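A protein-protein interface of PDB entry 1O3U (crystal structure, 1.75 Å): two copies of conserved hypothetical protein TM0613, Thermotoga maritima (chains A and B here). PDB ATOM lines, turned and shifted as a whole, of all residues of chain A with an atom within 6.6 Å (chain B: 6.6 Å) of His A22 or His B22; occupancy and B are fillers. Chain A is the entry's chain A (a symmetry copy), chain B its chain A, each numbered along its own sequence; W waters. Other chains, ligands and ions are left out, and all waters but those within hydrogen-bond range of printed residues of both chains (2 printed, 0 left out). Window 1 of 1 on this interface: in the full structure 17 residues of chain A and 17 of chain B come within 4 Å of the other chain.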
ATOM      1  N   LYS A  17      28.150  32.632 -19.962  1.00  0.00           N
ATOM      2  CA  LYS A  17      28.974  31.598 -20.590  1.00  0.00           C
ATOM      3  C   LYS A  17      28.404  30.210 -20.368  1.00  0.00           C
ATOM      4  O   LYS A  17      28.459  29.366 -21.265  1.00  0.00           O
ATOM      5  CB  LYS A  17      30.429  31.711 -20.120  1.00  0.00           C
ATOM      6  CG  LYS A  17      31.121  32.954 -20.695  1.00  0.00           C
ATOM      7  CD  LYS A  17      32.425  33.299 -19.962  1.00  0.00           C
ATOM      8  N   ASP A  18      27.810  29.983 -19.195  1.00  0.00           N
ATOM      9  CA  ASP A  18      27.115  28.730 -18.913  1.00  0.00           C
ATOM     10  C   ASP A  18      25.880  28.567 -19.785  1.00  0.00           C
ATOM     11  O   ASP A  18      25.662  27.476 -20.302  1.00  0.00           O
ATOM     12  CB  ASP A  18      26.700  28.613 -17.454  1.00  0.00           C
ATOM     13  CG  ASP A  18      27.869  28.462 -16.521  1.00  0.00           C
ATOM     14  OD1 ASP A  18      29.011  28.245 -16.993  1.00  0.00           O
ATOM     15  OD2 ASP A  18      27.726  28.552 -15.278  1.00  0.00           O
ATOM     16  N   ASP A  19      25.052  29.619 -19.909  1.00  0.00           N
ATOM     17  CA  ASP A  19      23.927  29.601 -20.855  1.00  0.00           C
ATOM     18  C   ASP A  19      24.382  29.275 -22.307  1.00  0.00           C
ATOM     19  O   ASP A  19      23.718  28.539 -23.035  1.00  0.00           O
ATOM     20  CB  ASP A  19      23.191  30.949 -20.893  1.00  0.00           C
ATOM     21  CG  ASP A  19      22.328  31.202 -19.660  1.00  0.00           C
ATOM     22  OD1 ASP A  19      21.985  30.252 -18.899  1.00  0.00           O
ATOM     23  OD2 ASP A  19      21.894  32.347 -19.431  1.00  0.00           O
ATOM     24  N   LEU A  20      25.494  29.862 -22.726  1.00  0.00           N
ATOM     25  CA  LEU A  20      26.043  29.591 -24.057  1.00  0.00           C
ATOM     26  C   LEU A  20      26.396  28.098 -24.180  1.00  0.00           C
ATOM     27  O   LEU A  20      26.074  27.465 -25.173  1.00  0.00           O
ATOM     28  CB  LEU A  20      27.268  30.457 -24.357  1.00  0.00           C
ATOM     29  CG  LEU A  20      27.791  30.391 -25.803  1.00  0.00           C
ATOM     30  CD1 LEU A  20      26.772  30.881 -26.767  1.00  0.00           C
ATOM     31  CD2 LEU A  20      29.119  31.122 -25.975  1.00  0.00           C
ATOM     32  N   GLU A  21      27.046  27.541 -23.160  1.00  0.00           N
ATOM     33  CA  GLU A  21      27.404  26.131 -23.184  1.00  0.00           C
ATOM     34  C   GLU A  21      26.153  25.277 -23.235  1.00  0.00           C
ATOM     35  O   GLU A  21      26.106  24.289 -23.973  1.00  0.00           O
ATOM     36  CB  GLU A  21      28.257  25.762 -22.001  1.00  0.00           C
ATOM     37  CG  GLU A  21      28.882  24.393 -22.134  1.00  0.00           C
ATOM     38  CD  GLU A  21      30.039  24.316 -23.138  1.00  0.00           C
ATOM     39  OE1 GLU A  21      30.518  25.348 -23.708  1.00  0.00           O
ATOM     40  OE2 GLU A  21      30.464  23.166 -23.382  1.00  0.00           O
ATOM     41  N   HIS A  22      25.134  25.676 -22.478  1.00  0.00           N
ATOM     42  CA  HIS A  22      23.819  25.024 -22.524  1.00  0.00           C
ATOM     43  C   HIS A  22      23.272  25.031 -23.949  1.00  0.00           C
ATOM     44  O   HIS A  22      22.815  24.002 -24.456  1.00  0.00           O
ATOM     45  CB  HIS A  22      22.802  25.682 -21.596  1.00  0.00           C
ATOM     46  CG  HIS A  22      21.683  24.766 -21.151  1.00  0.00           C
ATOM     47  ND1 HIS A  22      20.736  25.148 -20.221  1.00  0.00           N
ATOM     48  CD2 HIS A  22      21.393  23.478 -21.468  1.00  0.00           C
ATOM     49  CE1 HIS A  22      19.908  24.139 -20.003  1.00  0.00           C
ATOM     50  NE2 HIS A  22      20.292  23.116 -20.734  1.00  0.00           N
ATOM     51  N   ALA A  23      23.289  26.198 -24.596  1.00  0.00           N
ATOM     52  CA  ALA A  23      22.810  26.327 -25.962  1.00  0.00           C
ATOM     53  C   ALA A  23      23.543  25.368 -26.929  1.00  0.00           C
ATOM     54  O   ALA A  23      22.921  24.758 -27.802  1.00  0.00           O
ATOM     55  CB  ALA A  23      22.971  27.711 -26.423  1.00  0.00           C
ATOM     56  N   LYS A  24      24.864  25.312 -26.792  1.00  0.00           N
ATOM     57  CA  LYS A  24      25.687  24.488 -27.627  1.00  0.00           C
ATOM     58  C   LYS A  24      25.397  22.975 -27.410  1.00  0.00           C
ATOM     59  O   LYS A  24      25.419  22.194 -28.359  1.00  0.00           O
ATOM     60  CB  LYS A  24      27.145  24.819 -27.369  1.00  0.00           C
ATOM     61  CG  LYS A  24      27.573  26.154 -27.988  1.00  0.00           C
ATOM     62  CD  LYS A  24      29.029  26.369 -27.817  1.00  0.00           C
ATOM     63  CE  LYS A  24      29.391  27.736 -28.327  1.00  0.00           C
ATOM     64  NZ  LYS A  24      30.818  27.961 -28.267  1.00  0.00           N
ATOM     65  N   HIS A  25      25.105  22.607 -26.179  1.00  0.00           N
ATOM     66  CA  HIS A  25      24.716  21.242 -25.838  1.00  0.00           C
ATOM     67  C   HIS A  25      23.389  20.892 -26.467  1.00  0.00           C
ATOM     68  O   HIS A  25      23.240  19.818 -27.072  1.00  0.00           O
ATOM     69  CB  HIS A  25      24.622  21.100 -24.328  1.00  0.00           C
ATOM     70  CG  HIS A  25      24.412  19.689 -23.875  1.00  0.00           C
ATOM     71  ND1 HIS A  25      23.179  19.214 -23.491  1.00  0.00           N
ATOM     72  CD2 HIS A  25      25.275  18.652 -23.754  1.00  0.00           C
ATOM     73  CE1 HIS A  25      23.294  17.944 -23.138  1.00  0.00           C
ATOM     74  NE2 HIS A  25      24.553  17.575 -23.298  1.00  0.00           N
ATOM     75  N   ASP A  26      22.413  21.793 -26.329  1.00  0.00           N
ATOM     76  CA  ASP A  26      21.101  21.596 -26.962  1.00  0.00           C
ATOM     77  C   ASP A  26      21.250  21.517 -28.490  1.00  0.00           C
ATOM     78  O   ASP A  26      20.630  20.654 -29.130  1.00  0.00           O
ATOM     79  CB  ASP A  26      20.122  22.710 -26.613  1.00  0.00           C
ATOM     80  CG  ASP A  26      19.522  22.560 -25.201  1.00  0.00           C
ATOM     81  OD1 ASP A  26      19.296  21.420 -24.723  1.00  0.00           O
ATOM     82  OD2 ASP A  26      19.264  23.540 -24.530  1.00  0.00           O
ATOM     83  N   LEU A  27      22.085  22.385 -29.075  1.00  0.00           N
ATOM     84  CA  LEU A  27      22.324  22.340 -30.498  1.00  0.00           C
ATOM     85  C   LEU A  27      22.845  20.971 -30.952  1.00  0.00           C
ATOM     86  O   LEU A  27      22.373  20.426 -31.958  1.00  0.00           O
ATOM     87  CB  LEU A  27      23.294  23.423 -30.910  1.00  0.00           C
ATOM     88  CG  LEU A  27      23.644  23.546 -32.386  1.00  0.00           C
ATOM     89  CD1 LEU A  27      22.385  23.755 -33.237  1.00  0.00           C
ATOM     90  CD2 LEU A  27      24.606  24.699 -32.529  1.00  0.00           C
ATOM     91  N   TRP A  34      15.417  24.921 -28.074  1.00  0.00           N
ATOM     92  CA  TRP A  34      16.020  25.199 -26.782  1.00  0.00           C
ATOM     93  C   TRP A  34      17.353  25.924 -26.949  1.00  0.00           C
ATOM     94  O   TRP A  34      17.685  26.802 -26.146  1.00  0.00           O
ATOM     95  CB  TRP A  34      16.162  23.901 -25.984  1.00  0.00           C
ATOM     96  CG  TRP A  34      14.856  23.455 -25.399  1.00  0.00           C
ATOM     97  CD1 TRP A  34      14.216  22.276 -25.635  1.00  0.00           C
ATOM     98  CD2 TRP A  34      14.024  24.187 -24.488  1.00  0.00           C
ATOM     99  NE1 TRP A  34      13.041  22.222 -24.922  1.00  0.00           N
ATOM    100  CE2 TRP A  34      12.902  23.380 -24.195  1.00  0.00           C
ATOM    101  CE3 TRP A  34      14.121  25.444 -23.867  1.00  0.00           C
ATOM    102  CZ2 TRP A  34      11.886  23.793 -23.331  1.00  0.00           C
ATOM    103  CZ3 TRP A  34      13.129  25.846 -23.001  1.00  0.00           C
ATOM    104  CH2 TRP A  34      12.009  25.028 -22.747  1.00  0.00           C
ATOM    105  N   ALA A  35      18.087  25.611 -28.017  1.00  0.00           N
ATOM    106  CA  ALA A  35      19.342  26.288 -28.294  1.00  0.00           C
ATOM    107  C   ALA A  35      19.090  27.789 -28.501  1.00  0.00           C
ATOM    108  O   ALA A  35      19.842  28.611 -28.020  1.00  0.00           O
ATOM    109  CB  ALA A  35      20.044  25.686 -29.495  1.00  0.00           C
ATOM    110  N   PHE A  37      16.529  29.477 -27.252  1.00  0.00           N
ATOM    111  CA  PHE A  37      16.169  30.016 -25.934  1.00  0.00           C
ATOM    112  C   PHE A  37      17.402  30.342 -25.062  1.00  0.00           C
ATOM    113  O   PHE A  37      17.525  31.438 -24.512  1.00  0.00           O
ATOM    114  CB  PHE A  37      15.258  29.001 -25.239  1.00  0.00           C
ATOM    115  CG  PHE A  37      14.879  29.386 -23.851  1.00  0.00           C
ATOM    116  CD1 PHE A  37      13.938  30.368 -23.627  1.00  0.00           C
ATOM    117  CD2 PHE A  37      15.438  28.743 -22.763  1.00  0.00           C
ATOM    118  CE1 PHE A  37      13.567  30.721 -22.331  1.00  0.00           C
ATOM    119  CE2 PHE A  37      15.094  29.110 -21.473  1.00  0.00           C
ATOM    120  CZ  PHE A  37      14.141  30.070 -21.260  1.00  0.00           C
ATOM    121  N   SER A  38      18.309  29.379 -24.942  1.00  0.00           N
ATOM    122  CA  SER A  38      19.528  29.529 -24.153  1.00  0.00           C
ATOM    123  C   SER A  38      20.409  30.672 -24.697  1.00  0.00           C
ATOM    124  O   SER A  38      21.070  31.373 -23.941  1.00  0.00           O
ATOM    125  CB  SER A  38      20.333  28.246 -24.195  1.00  0.00           C
ATOM    126  OG  SER A  38      19.690  27.230 -23.456  1.00  0.00           O
ATOM    127  N   LYS B  17       9.031  29.831 -15.919  1.00  0.00           N
ATOM    128  CA  LYS B  17       8.306  28.639 -16.362  1.00  0.00           C
ATOM    129  C   LYS B  17       8.967  27.990 -17.563  1.00  0.00           C
ATOM    130  O   LYS B  17       9.005  26.761 -17.662  1.00  0.00           O
ATOM    131  CB  LYS B  17       6.831  28.970 -16.618  1.00  0.00           C
ATOM    132  CG  LYS B  17       6.071  29.245 -15.313  1.00  0.00           C
ATOM    133  CD  LYS B  17       4.721  29.936 -15.548  1.00  0.00           C
ATOM    134  N   ASP B  18       9.536  28.807 -18.452  1.00  0.00           N
ATOM    135  CA  ASP B  18      10.308  28.297 -19.581  1.00  0.00           C
ATOM    136  C   ASP B  18      11.583  27.607 -19.119  1.00  0.00           C
ATOM    137  O   ASP B  18      11.898  26.540 -19.639  1.00  0.00           O
ATOM    138  CB  ASP B  18      10.680  29.392 -20.569  1.00  0.00           C
ATOM    139  CG  ASP B  18       9.493  29.941 -21.312  1.00  0.00           C
ATOM    140  OD1 ASP B  18       8.387  29.355 -21.225  1.00  0.00           O
ATOM    141  OD2 ASP B  18       9.586  30.977 -22.014  1.00  0.00           O
ATOM    142  N   ASP B  19      12.336  28.225 -18.193  1.00  0.00           N
ATOM    143  CA  ASP B  19      13.491  27.557 -17.576  1.00  0.00           C
ATOM    144  C   ASP B  19      13.113  26.190 -16.939  1.00  0.00           C
ATOM    145  O   ASP B  19      13.853  25.212 -17.034  1.00  0.00           O
ATOM    146  CB  ASP B  19      14.127  28.419 -16.476  1.00  0.00           C
ATOM    147  CG  ASP B  19      14.927  29.601 -17.020  1.00  0.00           C
ATOM    148  OD1 ASP B  19      15.311  29.628 -18.223  1.00  0.00           O
ATOM    149  OD2 ASP B  19      15.267  30.523 -16.255  1.00  0.00           O
ATOM    150  N   LEU B  20      11.975  26.147 -16.258  1.00  0.00           N
ATOM    151  CA  LEU B  20      11.496  24.901 -15.656  1.00  0.00           C
ATOM    152  C   LEU B  20      11.255  23.850 -16.756  1.00  0.00           C
ATOM    153  O   LEU B  20      11.658  22.706 -16.617  1.00  0.00           O
ATOM    154  CB  LEU B  20      10.221  25.116 -14.836  1.00  0.00           C
ATOM    155  CG  LEU B  20       9.756  23.910 -14.002  1.00  0.00           C
ATOM    156  CD1 LEU B  20      10.768  23.537 -12.982  1.00  0.00           C
ATOM    157  CD2 LEU B  20       8.385  24.134 -13.371  1.00  0.00           C
ATOM    158  N   GLU B  21      10.612  24.252 -17.850  1.00  0.00           N
ATOM    159  CA  GLU B  21      10.359  23.330 -18.947  1.00  0.00           C
ATOM    160  C   GLU B  21      11.670  22.850 -19.537  1.00  0.00           C
ATOM    161  O   GLU B  21      11.814  21.664 -19.845  1.00  0.00           O
ATOM    162  CB  GLU B  21       9.494  23.961 -20.004  1.00  0.00           C
ATOM    163  CG  GLU B  21       8.975  22.961 -21.011  1.00  0.00           C
ATOM    164  CD  GLU B  21       7.862  22.046 -20.483  1.00  0.00           C
ATOM    165  OE1 GLU B  21       7.331  22.209 -19.339  1.00  0.00           O
ATOM    166  OE2 GLU B  21       7.531  21.109 -21.242  1.00  0.00           O
ATOM    167  N   HIS B  22      12.630  23.763 -19.664  1.00  0.00           N
ATOM    168  CA  HIS B  22      13.990  23.417 -20.098  1.00  0.00           C
ATOM    169  C   HIS B  22      14.584  22.350 -19.182  1.00  0.00           C
ATOM    170  O   HIS B  22      15.133  21.348 -19.652  1.00  0.00           O
ATOM    171  CB  HIS B  22      14.924  24.624 -20.129  1.00  0.00           C
ATOM    172  CG  HIS B  22      16.091  24.483 -21.083  1.00  0.00           C
ATOM    173  ND1 HIS B  22      16.974  25.514 -21.333  1.00  0.00           N
ATOM    174  CD2 HIS B  22      16.484  23.455 -21.879  1.00  0.00           C
ATOM    175  CE1 HIS B  22      17.865  25.117 -22.227  1.00  0.00           C
ATOM    176  NE2 HIS B  22      17.582  23.882 -22.581  1.00  0.00           N
ATOM    177  N   ALA B  23      14.505  22.570 -17.868  1.00  0.00           N
ATOM    178  CA  ALA B  23      15.021  21.620 -16.897  1.00  0.00           C
ATOM    179  C   ALA B  23      14.394  20.216 -17.066  1.00  0.00           C
ATOM    180  O   ALA B  23      15.090  19.201 -16.974  1.00  0.00           O
ATOM    181  CB  ALA B  23      14.776  22.110 -15.536  1.00  0.00           C
ATOM    182  N   LYS B  24      13.076  20.193 -17.242  1.00  0.00           N
ATOM    183  CA  LYS B  24      12.344  18.969 -17.391  1.00  0.00           C
ATOM    184  C   LYS B  24      12.737  18.218 -18.696  1.00  0.00           C
ATOM    185  O   LYS B  24      12.804  16.991 -18.712  1.00  0.00           O
ATOM    186  CB  LYS B  24      10.858  19.270 -17.344  1.00  0.00           C
ATOM    187  CG  LYS B  24      10.358  19.587 -15.932  1.00  0.00           C
ATOM    188  CD  LYS B  24       8.884  19.748 -15.922  1.00  0.00           C
ATOM    189  CE  LYS B  24       8.442  20.174 -14.550  1.00  0.00           C
ATOM    190  NZ  LYS B  24       7.000  20.257 -14.462  1.00  0.00           N
ATOM    191  N   HIS B  25      13.012  18.971 -19.741  1.00  0.00           N
ATOM    192  CA  HIS B  25      13.487  18.416 -21.006  1.00  0.00           C
ATOM    193  C   HIS B  25      14.857  17.805 -20.839  1.00  0.00           C
ATOM    194  O   HIS B  25      15.104  16.675 -21.293  1.00  0.00           O
ATOM    195  CB  HIS B  25      13.538  19.511 -22.057  1.00  0.00           C
ATOM    196  CG  HIS B  25      13.834  19.002 -23.434  1.00  0.00           C
ATOM    197  ND1 HIS B  25      15.083  19.097 -24.001  1.00  0.00           N
ATOM    198  CD2 HIS B  25      13.045  18.389 -24.348  1.00  0.00           C
ATOM    199  CE1 HIS B  25      15.049  18.574 -25.216  1.00  0.00           C
ATOM    200  NE2 HIS B  25      13.826  18.127 -25.447  1.00  0.00           N
ATOM    201  N   ASP B  26      15.758  18.543 -20.188  1.00  0.00           N
ATOM    202  CA  ASP B  26      17.103  18.022 -19.901  1.00  0.00           C
ATOM    203  C   ASP B  26      17.015  16.771 -19.012  1.00  0.00           C
ATOM    204  O   ASP B  26      17.718  15.780 -19.264  1.00  0.00           O
ATOM    205  CB  ASP B  26      17.987  19.058 -19.216  1.00  0.00           C
ATOM    206  CG  ASP B  26      18.545  20.110 -20.195  1.00  0.00           C
ATOM    207  OD1 ASP B  26      18.836  19.790 -21.375  1.00  0.00           O
ATOM    208  OD2 ASP B  26      18.709  21.261 -19.841  1.00  0.00           O
ATOM    209  N   LEU B  27      16.139  16.794 -17.998  1.00  0.00           N
ATOM    210  CA  LEU B  27      15.954  15.640 -17.153  1.00  0.00           C
ATOM    211  C   LEU B  27      15.550  14.396 -17.955  1.00  0.00           C
ATOM    212  O   LEU B  27      16.096  13.307 -17.734  1.00  0.00           O
ATOM    213  CB  LEU B  27      14.922  15.921 -16.085  1.00  0.00           C
ATOM    214  CG  LEU B  27      14.617  14.821 -15.078  1.00  0.00           C
ATOM    215  CD1 LEU B  27      15.885  14.380 -14.339  1.00  0.00           C
ATOM    216  CD2 LEU B  27      13.578  15.357 -14.124  1.00  0.00           C
ATOM    217  N   TRP B  34      22.566  19.636 -16.414  1.00  0.00           N
ATOM    218  CA  TRP B  34      21.900  20.773 -17.027  1.00  0.00           C
ATOM    219  C   TRP B  34      20.524  20.997 -16.403  1.00  0.00           C
ATOM    220  O   TRP B  34      20.101  22.145 -16.233  1.00  0.00           O
ATOM    221  CB  TRP B  34      21.824  20.578 -18.542  1.00  0.00           C
ATOM    222  CG  TRP B  34      23.139  20.851 -19.210  1.00  0.00           C
ATOM    223  CD1 TRP B  34      23.871  19.980 -19.960  1.00  0.00           C
ATOM    224  CD2 TRP B  34      23.883  22.077 -19.180  1.00  0.00           C
ATOM    225  NE1 TRP B  34      25.021  20.589 -20.406  1.00  0.00           N
ATOM    226  CE2 TRP B  34      25.049  21.885 -19.953  1.00  0.00           C
ATOM    227  CE3 TRP B  34      23.673  23.336 -18.592  1.00  0.00           C
ATOM    228  CZ2 TRP B  34      26.001  22.890 -20.136  1.00  0.00           C
ATOM    229  CZ3 TRP B  34      24.602  24.334 -18.785  1.00  0.00           C
ATOM    230  CH2 TRP B  34      25.768  24.105 -19.543  1.00  0.00           C
ATOM    231  N   ALA B  35      19.853  19.916 -16.006  1.00  0.00           N
ATOM    232  CA  ALA B  35      18.562  20.030 -15.348  1.00  0.00           C
ATOM    233  C   ALA B  35      18.711  20.820 -14.040  1.00  0.00           C
ATOM    234  O   ALA B  35      17.885  21.652 -13.726  1.00  0.00           O
ATOM    235  CB  ALA B  35      17.948  18.668 -15.092  1.00  0.00           C
ATOM    236  N   PHE B  37      21.098  23.030 -13.415  1.00  0.00           N
ATOM    237  CA  PHE B  37      21.370  24.419 -13.806  1.00  0.00           C
ATOM    238  C   PHE B  37      20.088  25.213 -14.140  1.00  0.00           C
ATOM    239  O   PHE B  37      19.866  26.314 -13.634  1.00  0.00           O
ATOM    240  CB  PHE B  37      22.329  24.396 -15.001  1.00  0.00           C
ATOM    241  CG  PHE B  37      22.631  25.745 -15.555  1.00  0.00           C
ATOM    242  CD1 PHE B  37      23.489  26.599 -14.896  1.00  0.00           C
ATOM    243  CD2 PHE B  37      22.081  26.153 -16.756  1.00  0.00           C
ATOM    244  CE1 PHE B  37      23.788  27.855 -15.418  1.00  0.00           C
ATOM    245  CE2 PHE B  37      22.353  27.413 -17.264  1.00  0.00           C
ATOM    246  CZ  PHE B  37      23.225  28.245 -16.616  1.00  0.00           C
ATOM    247  N   SER B  38      19.249  24.641 -14.998  1.00  0.00           N
ATOM    248  CA  SER B  38      17.995  25.261 -15.417  1.00  0.00           C
ATOM    249  C   SER B  38      17.055  25.483 -14.216  1.00  0.00           C
ATOM    250  O   SER B  38      16.319  26.461 -14.166  1.00  0.00           O
ATOM    251  CB  SER B  38      17.289  24.371 -16.419  1.00  0.00           C
ATOM    252  OG  SER B  38      17.977  24.362 -17.651  1.00  0.00           O
HETATM  253  O   HOH W   1      20.819  20.503 -22.890  1.00  0.00           O
HETATM  254  O   HOH W   2      17.322  20.538 -23.289  1.00  0.00           O
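NE2 of His B22 sits at hydrogen-bond distance from OD2 of Asp A26 (2.6 Å).
NE2 of His B22 is in hydrogen-bond range of NE2 of His A22, 3.4 Å away.
OD2 of Asp B26 lies within hydrogen-bond range of NE2 of His A22 (2.6 Å).
The backbone carbonyl oxygen of Trp A34 lies within hydrogen-bond range of the side-chain hydroxyl of Ser A38.
OG of Ser B38 lies within hydrogen-bond range of O of Trp B34 (3.4 Å).
Phe B37 touches Asp A19 (CZ to OD1, 3.3 Å).
Glu A21 touches Trp B34 (CG to CZ2, 3.8 Å).
CH2 of Trp B34 touches N of His A22, at 3.4 Å.
His A22 touches Ser B38 (CE1 to OG, 3.1 Å).
His A25 touches Trp B34 (CG to NE1, 3.6 Å).
Trp A34 touches Glu B21.
N of His B22 touches CH2 of Trp A34, 3.4 Å away.
NE1 of Trp A34 touches CG of His B25, 3.6 Å away.
Phe A37 touches Asp B18 (CZ to CB, 3.6 Å).
Ser A38 touches His B22 (OG to CE1, 3.1 Å).
His A22 touches just these residues of chain B: His B22 (3.2 Å), Asp B26 (2.6 Å), Trp B34 (3.4 Å), Phe B37 (3.9 Å) and Ser B38 (3.1 Å).
His B22 touches just these residues of chain A: His A22, Asp A26, Trp A34, Phe A37 and Ser A38.
Of the printed residues of chain B, His A25 touches Trp B34.
Of the printed residues of chain A, Asp B26 touches His A22 (2.6 Å) and Asp A26 (3.8 Å).
Of the printed residues of chain A, Ser B38 touches His A22 (3.1 Å).
Lys B24 touches none of the printed residues of chain A.
The nearest residue of chain B that does not touch His A22 is Ala B35 (5.7 Å).
The nearest printed residue of chain B that does not touch Asp A26 is His B25 (4.9 Å).
Of the 15 printed residues of chain A, 9 touch a printed residue of chain B.
Hydrophobic or aromatic side chains of chain A within 4 Å of the printed part of chain B: His A22, His A25, Trp A34 and Phe A37.
Among the printed residues, 20 pairs touch across the chains.
Asp A18 touches Phe B37, and with the chains exchanged Phe A37 touches Asp B18.
Asp A19 touches Phe B37, and with the chains exchanged Phe A37 touches Asp B19.
His B22 touches its own counterpart, His A22.
His A22 touches Asp B26, and with the chains exchanged Asp A26 touches His B22.
15 positions are printed for both chains.
Of the 20 pairs that touch across the chains among the printed residues, 20 have their exchanged pair printed and touching as well.
Water W2 lies within hydrogen-bond range of OD1 of Asp B26 (2.6 Å), OD1 of Asp A26 (2.6 Å), ND1 of His B25 (2.8 Å) and NE2 of His B22 (3.4 Å).
Water W1 lies within hydrogen-bond range of the side-chain carboxylate (OD1) of Asp A26 (2.6 Å), the side-chain carboxylate (OD1) of Asp B26 (2.6 Å), a ring nitrogen (ND1) of His A25 (2.8 Å) and a ring nitrogen (NE2) of His A22 (3.4 Å).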
